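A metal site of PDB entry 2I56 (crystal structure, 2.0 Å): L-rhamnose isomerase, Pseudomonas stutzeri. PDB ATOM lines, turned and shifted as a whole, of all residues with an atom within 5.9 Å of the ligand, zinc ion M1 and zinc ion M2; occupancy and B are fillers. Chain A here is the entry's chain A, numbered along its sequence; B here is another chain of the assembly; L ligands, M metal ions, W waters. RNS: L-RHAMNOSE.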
ATOM      1  N   TRP A  57      26.435  26.098 -17.471  1.00  0.00           N
ATOM      2  CA  TRP A  57      26.069  25.960 -16.062  1.00  0.00           C
ATOM      3  C   TRP A  57      27.094  25.238 -15.180  1.00  0.00           C
ATOM      4  O   TRP A  57      26.927  25.160 -13.960  1.00  0.00           O
ATOM      5  CB  TRP A  57      24.691  25.270 -15.938  1.00  0.00           C
ATOM      6  CG  TRP A  57      24.620  23.880 -16.489  1.00  0.00           C
ATOM      7  CD1 TRP A  57      24.815  22.711 -15.816  1.00  0.00           C
ATOM      8  CD2 TRP A  57      24.316  23.506 -17.840  1.00  0.00           C
ATOM      9  NE1 TRP A  57      24.648  21.636 -16.647  1.00  0.00           N
ATOM     10  CE2 TRP A  57      24.344  22.094 -17.903  1.00  0.00           C
ATOM     11  CE3 TRP A  57      24.019  24.235 -19.000  1.00  0.00           C
ATOM     12  CZ2 TRP A  57      24.078  21.395 -19.087  1.00  0.00           C
ATOM     13  CZ3 TRP A  57      23.760  23.531 -20.179  1.00  0.00           C
ATOM     14  CH2 TRP A  57      23.801  22.134 -20.211  1.00  0.00           C
ATOM     15  N   HIS A 101      21.791  27.446 -21.403  1.00  0.00           N
ATOM     16  CA  HIS A 101      20.606  27.020 -20.669  1.00  0.00           C
ATOM     17  C   HIS A 101      19.712  28.249 -20.470  1.00  0.00           C
ATOM     18  O   HIS A 101      20.171  29.284 -20.008  1.00  0.00           O
ATOM     19  CB  HIS A 101      21.024  26.440 -19.311  1.00  0.00           C
ATOM     20  CG  HIS A 101      20.216  25.260 -18.896  1.00  0.00           C
ATOM     21  ND1 HIS A 101      18.849  25.321 -18.702  1.00  0.00           N
ATOM     22  CD2 HIS A 101      20.577  23.981 -18.631  1.00  0.00           C
ATOM     23  CE1 HIS A 101      18.411  24.126 -18.340  1.00  0.00           C
ATOM     24  NE2 HIS A 101      19.430  23.295 -18.295  1.00  0.00           N
ATOM     25  N   TRP A 104      18.483  30.772 -17.556  1.00  0.00           N
ATOM     26  CA  TRP A 104      19.713  31.196 -16.867  1.00  0.00           C
ATOM     27  C   TRP A 104      20.602  32.086 -17.723  1.00  0.00           C
ATOM     28  O   TRP A 104      21.093  33.116 -17.271  1.00  0.00           O
ATOM     29  CB  TRP A 104      20.550  29.998 -16.409  1.00  0.00           C
ATOM     30  CG  TRP A 104      19.891  29.102 -15.399  1.00  0.00           C
ATOM     31  CD1 TRP A 104      18.889  29.430 -14.542  1.00  0.00           C
ATOM     32  CD2 TRP A 104      20.207  27.726 -15.152  1.00  0.00           C
ATOM     33  NE1 TRP A 104      18.561  28.346 -13.763  1.00  0.00           N
ATOM     34  CE2 TRP A 104      19.351  27.279 -14.117  1.00  0.00           C
ATOM     35  CE3 TRP A 104      21.131  26.826 -15.693  1.00  0.00           C
ATOM     36  CZ2 TRP A 104      19.389  25.980 -13.615  1.00  0.00           C
ATOM     37  CZ3 TRP A 104      21.171  25.520 -15.199  1.00  0.00           C
ATOM     38  CH2 TRP A 104      20.303  25.112 -14.171  1.00  0.00           C
ATOM     39  N   ASN A 127      19.374  24.240 -24.168  1.00  0.00           N
ATOM     40  CA  ASN A 127      18.776  23.416 -23.128  1.00  0.00           C
ATOM     41  C   ASN A 127      17.614  24.185 -22.512  1.00  0.00           C
ATOM     42  O   ASN A 127      17.788  25.323 -22.075  1.00  0.00           O
ATOM     43  CB  ASN A 127      19.806  23.104 -22.037  1.00  0.00           C
ATOM     44  CG  ASN A 127      20.945  22.231 -22.543  1.00  0.00           C
ATOM     45  OD1 ASN A 127      20.884  21.010 -22.468  1.00  0.00           O
ATOM     46  ND2 ASN A 127      21.977  22.863 -23.081  1.00  0.00           N
ATOM     47  N   SER A 128      16.434  23.572 -22.475  1.00  0.00           N
ATOM     48  CA  SER A 128      15.276  24.234 -21.894  1.00  0.00           C
ATOM     49  C   SER A 128      15.207  23.971 -20.386  1.00  0.00           C
ATOM     50  O   SER A 128      15.835  23.038 -19.884  1.00  0.00           O
ATOM     51  CB  SER A 128      13.986  23.760 -22.564  1.00  0.00           C
ATOM     52  OG  SER A 128      13.852  22.357 -22.465  1.00  0.00           O
ATOM     53  N   PHE A 131      12.057  22.636 -15.078  1.00  0.00           N
ATOM     54  CA  PHE A 131      12.228  21.854 -13.853  1.00  0.00           C
ATOM     55  C   PHE A 131      12.359  22.806 -12.656  1.00  0.00           C
ATOM     56  O   PHE A 131      12.642  22.385 -11.526  1.00  0.00           O
ATOM     57  CB  PHE A 131      13.440  20.914 -13.962  1.00  0.00           C
ATOM     58  CG  PHE A 131      14.729  21.587 -14.346  1.00  0.00           C
ATOM     59  CD1 PHE A 131      15.431  22.371 -13.436  1.00  0.00           C
ATOM     60  CD2 PHE A 131      15.252  21.424 -15.634  1.00  0.00           C
ATOM     61  CE1 PHE A 131      16.633  22.977 -13.798  1.00  0.00           C
ATOM     62  CE2 PHE A 131      16.457  22.024 -16.003  1.00  0.00           C
ATOM     63  CZ  PHE A 131      17.149  22.807 -15.082  1.00  0.00           C
ATOM     64  N   THR A 177      17.987  20.332 -26.387  1.00  0.00           N
ATOM     65  CA  THR A 177      17.999  19.202 -25.466  1.00  0.00           C
ATOM     66  C   THR A 177      16.918  19.437 -24.435  1.00  0.00           C
ATOM     67  O   THR A 177      16.841  20.510 -23.835  1.00  0.00           O
ATOM     68  CB  THR A 177      19.341  19.084 -24.733  1.00  0.00           C
ATOM     69  OG1 THR A 177      20.364  18.767 -25.681  1.00  0.00           O
ATOM     70  CG2 THR A 177      19.261  17.993 -23.663  1.00  0.00           C
ATOM     71  N   TRP A 179      15.439  18.017 -20.924  1.00  0.00           N
ATOM     72  CA  TRP A 179      15.472  17.192 -19.736  1.00  0.00           C
ATOM     73  C   TRP A 179      14.501  17.848 -18.768  1.00  0.00           C
ATOM     74  O   TRP A 179      14.588  19.055 -18.527  1.00  0.00           O
ATOM     75  CB  TRP A 179      16.845  17.165 -19.062  1.00  0.00           C
ATOM     76  CG  TRP A 179      16.768  16.426 -17.754  1.00  0.00           C
ATOM     77  CD1 TRP A 179      16.595  15.080 -17.580  1.00  0.00           C
ATOM     78  CD2 TRP A 179      16.705  17.005 -16.440  1.00  0.00           C
ATOM     79  NE1 TRP A 179      16.416  14.788 -16.242  1.00  0.00           N
ATOM     80  CE2 TRP A 179      16.484  15.952 -15.522  1.00  0.00           C
ATOM     81  CE3 TRP A 179      16.816  18.316 -15.948  1.00  0.00           C
ATOM     82  CZ2 TRP A 179      16.360  16.165 -14.146  1.00  0.00           C
ATOM     83  CZ3 TRP A 179      16.685  18.523 -14.568  1.00  0.00           C
ATOM     84  CH2 TRP A 179      16.460  17.455 -13.692  1.00  0.00           C
ATOM     85  N   GLU A 219      16.313  13.513 -22.935  1.00  0.00           N
ATOM     86  CA  GLU A 219      17.245  12.889 -22.001  1.00  0.00           C
ATOM     87  C   GLU A 219      16.560  12.130 -20.870  1.00  0.00           C
ATOM     88  O   GLU A 219      15.796  12.718 -20.095  1.00  0.00           O
ATOM     89  CB  GLU A 219      18.159  13.981 -21.412  1.00  0.00           C
ATOM     90  CG  GLU A 219      19.107  13.514 -20.321  1.00  0.00           C
ATOM     91  CD  GLU A 219      20.059  14.623 -19.874  1.00  0.00           C
ATOM     92  OE1 GLU A 219      19.777  15.803 -20.156  1.00  0.00           O
ATOM     93  OE2 GLU A 219      21.086  14.317 -19.228  1.00  0.00           O
ATOM     94  N   LYS A 221      16.317   9.793 -17.336  1.00  0.00           N
ATOM     95  CA  LYS A 221      16.932   9.809 -16.017  1.00  0.00           C
ATOM     96  C   LYS A 221      16.088   8.935 -15.095  1.00  0.00           C
ATOM     97  O   LYS A 221      14.876   9.124 -15.000  1.00  0.00           O
ATOM     98  CB  LYS A 221      17.012  11.235 -15.466  1.00  0.00           C
ATOM     99  CG  LYS A 221      17.873  11.355 -14.199  1.00  0.00           C
ATOM    100  CD  LYS A 221      17.958  12.798 -13.697  1.00  0.00           C
ATOM    101  CE  LYS A 221      18.850  12.892 -12.453  1.00  0.00           C
ATOM    102  NZ  LYS A 221      18.930  14.283 -11.913  1.00  0.00           N
ATOM    103  N   GLU A 224      15.338  11.551  -9.489  1.00  0.00           N
ATOM    104  CA  GLU A 224      15.834  12.866  -9.071  1.00  0.00           C
ATOM    105  C   GLU A 224      15.591  13.888 -10.178  1.00  0.00           C
ATOM    106  O   GLU A 224      16.201  13.817 -11.235  1.00  0.00           O
ATOM    107  CB  GLU A 224      17.338  12.886  -8.727  1.00  0.00           C
ATOM    108  CG  GLU A 224      17.779  14.283  -8.247  1.00  0.00           C
ATOM    109  CD  GLU A 224      19.273  14.523  -8.278  1.00  0.00           C
ATOM    110  OE1 GLU A 224      19.951  14.035  -9.207  1.00  0.00           O
ATOM    111  OE2 GLU A 224      19.771  15.224  -7.370  1.00  0.00           O
ATOM    112  N   LEU A 252      19.464  11.210 -25.847  1.00  0.00           N
ATOM    113  CA  LEU A 252      20.722  11.663 -25.261  1.00  0.00           C
ATOM    114  C   LEU A 252      21.002  10.806 -24.035  1.00  0.00           C
ATOM    115  O   LEU A 252      20.126  10.616 -23.187  1.00  0.00           O
ATOM    116  CB  LEU A 252      20.607  13.146 -24.904  1.00  0.00           C
ATOM    117  CG  LEU A 252      21.887  13.831 -24.435  1.00  0.00           C
ATOM    118  CD1 LEU A 252      21.943  15.243 -25.005  1.00  0.00           C
ATOM    119  CD2 LEU A 252      21.945  13.820 -22.910  1.00  0.00           C
ATOM    120  N   ASP A 254      23.042  10.399 -20.667  1.00  0.00           N
ATOM    121  CA  ASP A 254      23.842  11.053 -19.641  1.00  0.00           C
ATOM    122  C   ASP A 254      24.331   9.910 -18.766  1.00  0.00           C
ATOM    123  O   ASP A 254      23.543   9.226 -18.112  1.00  0.00           O
ATOM    124  CB  ASP A 254      22.992  12.033 -18.828  1.00  0.00           C
ATOM    125  CG  ASP A 254      23.809  12.779 -17.788  1.00  0.00           C
ATOM    126  OD1 ASP A 254      23.701  14.025 -17.716  1.00  0.00           O
ATOM    127  OD2 ASP A 254      24.552  12.125 -17.034  1.00  0.00           O
ATOM    128  N   HIS A 257      22.857   8.799 -15.306  1.00  0.00           N
ATOM    129  CA  HIS A 257      21.407   8.671 -15.191  1.00  0.00           C
ATOM    130  C   HIS A 257      20.822   7.266 -15.220  1.00  0.00           C
ATOM    131  O   HIS A 257      19.620   7.098 -15.473  1.00  0.00           O
ATOM    132  CB  HIS A 257      20.726   9.489 -16.294  1.00  0.00           C
ATOM    133  CG  HIS A 257      20.873  10.966 -16.134  1.00  0.00           C
ATOM    134  ND1 HIS A 257      20.096  11.869 -16.829  1.00  0.00           N
ATOM    135  CD2 HIS A 257      21.686  11.704 -15.349  1.00  0.00           C
ATOM    136  CE1 HIS A 257      20.431  13.100 -16.489  1.00  0.00           C
ATOM    137  NE2 HIS A 257      21.402  13.021 -15.592  1.00  0.00           N
ATOM    138  N   HIS A 281      26.072  13.126 -22.554  1.00  0.00           N
ATOM    139  CA  HIS A 281      26.285  14.074 -21.484  1.00  0.00           C
ATOM    140  C   HIS A 281      27.317  13.321 -20.654  1.00  0.00           C
ATOM    141  O   HIS A 281      26.978  12.385 -19.926  1.00  0.00           O
ATOM    142  CB  HIS A 281      25.020  14.320 -20.661  1.00  0.00           C
ATOM    143  CG  HIS A 281      24.265  15.547 -21.076  1.00  0.00           C
ATOM    144  ND1 HIS A 281      23.270  16.113 -20.293  1.00  0.00           N
ATOM    145  CD2 HIS A 281      24.352  16.321 -22.188  1.00  0.00           C
ATOM    146  CE1 HIS A 281      22.779  17.170 -20.910  1.00  0.00           C
ATOM    147  NE2 HIS A 281      23.415  17.327 -22.054  1.00  0.00           N
ATOM    148  N   ASN A 283      30.161  12.610 -17.797  1.00  0.00           N
ATOM    149  CA  ASN A 283      30.426  12.857 -16.388  1.00  0.00           C
ATOM    150  C   ASN A 283      30.745  11.488 -15.797  1.00  0.00           C
ATOM    151  O   ASN A 283      30.779  10.489 -16.518  1.00  0.00           O
ATOM    152  CB  ASN A 283      29.209  13.464 -15.667  1.00  0.00           C
ATOM    153  CG  ASN A 283      27.904  12.748 -15.966  1.00  0.00           C
ATOM    154  OD1 ASN A 283      27.791  11.528 -15.805  1.00  0.00           O
ATOM    155  ND2 ASN A 283      26.909  13.510 -16.403  1.00  0.00           N
ATOM    156  N   ASP A 289      23.311  10.138  -9.701  1.00  0.00           N
ATOM    157  CA  ASP A 289      23.659  11.120 -10.731  1.00  0.00           C
ATOM    158  C   ASP A 289      24.606  12.104 -10.051  1.00  0.00           C
ATOM    159  O   ASP A 289      24.279  13.278  -9.864  1.00  0.00           O
ATOM    160  CB  ASP A 289      22.402  11.827 -11.236  1.00  0.00           C
ATOM    161  CG  ASP A 289      22.715  12.908 -12.250  1.00  0.00           C
ATOM    162  OD1 ASP A 289      23.694  12.763 -13.007  1.00  0.00           O
ATOM    163  OD2 ASP A 289      21.958  13.907 -12.300  1.00  0.00           O
ATOM    164  N   ASP A 291      27.298  13.551 -11.066  1.00  0.00           N
ATOM    165  CA  ASP A 291      27.837  14.622 -11.910  1.00  0.00           C
ATOM    166  C   ASP A 291      29.300  14.971 -11.633  1.00  0.00           C
ATOM    167  O   ASP A 291      29.676  16.143 -11.662  1.00  0.00           O
ATOM    168  CB  ASP A 291      26.974  15.875 -11.785  1.00  0.00           C
ATOM    169  CG  ASP A 291      25.589  15.687 -12.378  1.00  0.00           C
ATOM    170  OD1 ASP A 291      25.486  14.944 -13.374  1.00  0.00           O
ATOM    171  OD2 ASP A 291      24.611  16.282 -11.883  1.00  0.00           O
ATOM    172  N   ASP A 327      28.271  17.337 -18.899  1.00  0.00           N
ATOM    173  CA  ASP A 327      27.231  17.807 -18.006  1.00  0.00           C
ATOM    174  C   ASP A 327      27.678  17.422 -16.605  1.00  0.00           C
ATOM    175  O   ASP A 327      27.444  16.302 -16.157  1.00  0.00           O
ATOM    176  CB  ASP A 327      25.870  17.157 -18.308  1.00  0.00           C
ATOM    177  CG  ASP A 327      24.762  17.669 -17.403  1.00  0.00           C
ATOM    178  OD1 ASP A 327      25.042  18.541 -16.552  1.00  0.00           O
ATOM    179  OD2 ASP A 327      23.607  17.215 -17.543  1.00  0.00           O
ATOM    180  N   ARG B  65      18.230  19.763  -5.416  1.00  0.00           N
ATOM    181  CA  ARG B  65      19.242  20.688  -5.897  1.00  0.00           C
ATOM    182  C   ARG B  65      18.785  21.424  -7.153  1.00  0.00           C
ATOM    183  O   ARG B  65      19.444  22.372  -7.595  1.00  0.00           O
ATOM    184  CB  ARG B  65      20.558  19.962  -6.187  1.00  0.00           C
ATOM    185  CG  ARG B  65      20.446  18.902  -7.257  1.00  0.00           C
ATOM    186  CD  ARG B  65      21.816  18.341  -7.615  1.00  0.00           C
ATOM    187  NE  ARG B  65      21.696  17.096  -8.368  1.00  0.00           N
ATOM    188  CZ  ARG B  65      22.542  16.724  -9.331  1.00  0.00           C
ATOM    189  NH1 ARG B  65      23.568  17.501  -9.657  1.00  0.00           N
ATOM    190  NH2 ARG B  65      22.331  15.587  -9.974  1.00  0.00           N
ATOM    191  N   PHE B  66      17.678  20.997  -7.749  1.00  0.00           N
ATOM    192  CA  PHE B  66      17.170  21.645  -8.954  1.00  0.00           C
ATOM    193  C   PHE B  66      16.116  22.693  -8.657  1.00  0.00           C
ATOM    194  O   PHE B  66      15.979  23.657  -9.402  1.00  0.00           O
ATOM    195  CB  PHE B  66      16.581  20.603  -9.905  1.00  0.00           C
ATOM    196  CG  PHE B  66      17.596  19.626 -10.423  1.00  0.00           C
ATOM    197  CD1 PHE B  66      18.478  19.985 -11.435  1.00  0.00           C
ATOM    198  CD2 PHE B  66      17.693  18.351  -9.869  1.00  0.00           C
ATOM    199  CE1 PHE B  66      19.444  19.096 -11.893  1.00  0.00           C
ATOM    200  CE2 PHE B  66      18.657  17.457 -10.311  1.00  0.00           C
ATOM    201  CZ  PHE B  66      19.539  17.827 -11.332  1.00  0.00           C
HETATM  202  C1  RNS L   1      19.729  16.562 -14.904  1.00  0.00           C
HETATM  203  C2  RNS L   1      20.219  16.439 -16.336  1.00  0.00           C
HETATM  204  C3  RNS L   1      20.093  17.776 -17.074  1.00  0.00           C
HETATM  205  C4  RNS L   1      20.603  18.940 -16.215  1.00  0.00           C
HETATM  206  C5  RNS L   1      20.729  20.203 -17.064  1.00  0.00           C
HETATM  207  C6  RNS L   1      21.145  21.371 -16.172  1.00  0.00           C
HETATM  208  O1  RNS L   1      20.017  15.692 -14.079  1.00  0.00           O
HETATM  209  O2  RNS L   1      21.576  16.016 -16.350  1.00  0.00           O
HETATM  210  O3  RNS L   1      20.819  17.710 -18.293  1.00  0.00           O
HETATM  211  O4  RNS L   1      21.867  18.619 -15.651  1.00  0.00           O
HETATM  212  O5  RNS L   1      19.495  20.498 -17.689  1.00  0.00           O
HETATM  213 ZN    ZN M   1      22.505  15.716 -18.466  1.00  0.00          ZN
HETATM  214 ZN    ZN M   2      21.906  14.685 -14.350  1.00  0.00          ZN
HETATM  215  O   HOH W   1      22.320  17.021 -13.333  1.00  0.00           O
HETATM  216  O   HOH W   2      23.782  14.718 -15.125  1.00  0.00           O
HETATM  217  O   HOH W   3      19.309  19.920 -20.219  1.00  0.00           O
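Water W1 bridges the side-chain carboxylate (OD2) of Asp 291 and an oxygen (O4) of the ligand. Water W3 lies within hydrogen-bond range of an oxygen (O5) of the ligand and the side-chain amide oxygen of Asn 127.
Zinc ion M1 is bound by a ring nitrogen (ND1) of His 281 (2.0 Å), the side-chain carboxylate (OD2) of Asp 327 (2.1 Å), the side-chain carboxylate (OE2) of Glu 219 (2.1 Å), the side-chain carboxylate (OD1) of Asp 254 (2.2 Å) and an oxygen (O2) of the ligand (2.3 Å). Zinc ion M1 has five donor atoms within binding distance. Slightly farther from zinc ion M1 lies an oxygen (O3) of the ligand (2.6 Å).
The side-chain carboxylate of Asp 327 sits at hydrogen-bond distance from the indole nitrogen of Trp 57 (3.1 Å). The side-chain amide nitrogen (ND2) of Asn 283 is in hydrogen-bond range of the backbone carbonyl oxygen (O) of Asp 327. NZ of Lys 221 lies close to OD2 of Asp 289. O of Asp 289 sits at hydrogen-bond distance from NH2 of Arg 65 of chain B, 3.0 Å away. OD2 of Asp 254 lies within hydrogen-bond range of ND2 of Asn 283, at 2.8 Å. OE1 of Glu 224 is in salt-bridge range of NZ of Lys 221, 2.9 Å away. NH1 of Arg 65 of chain B is in salt-bridge range of OD2 of Asp 291.
Zinc ion M2 is bound by water W2 (2.0 Å), NE2 of His 257 (2.1 Å), O1 of the ligand (2.2 Å), OD2 of Asp 289 (2.2 Å), O2 of the ligand (2.4 Å) and water W1 (2.6 Å). Zinc ion M2 has six donor atoms within binding distance.
Residues that only touch zinc ion M2: Lys 221 and Asp 291. Of the 21 residues printed, 5 come within 4 Å of zinc ion M2.
The side-chain amino group (NZ) of Lys 221 sits close to an oxygen (O1) of the ligand (2.8 Å). A ring nitrogen (NE2) of His 101 is in hydrogen-bond range of an oxygen (O5) of the ligand (2.9 Å).
Merely in contact with the ligand: Trp 57 (3.5 Å), Phe 131 (3.8 Å), Trp 179 (3.4 Å) and Phe 66 of chain B (3.5 Å). Hydrophobic or aromatic side chains that line the ligand: Trp 57, His 101, Phe 131, Trp 179, His 257, His 281 and Phe 66 of chain B. 12 residues have an atom within 4 Å of the ligand: Trp 57, His 101, Phe 131, Trp 179, Glu 219, Lys 221, Asp 254, His 257, His 281, Asp 289, Asp 327 and Phe 66 of chain B. The nearest printed residue that does not touch the ligand is Trp 104 (4.3 Å).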
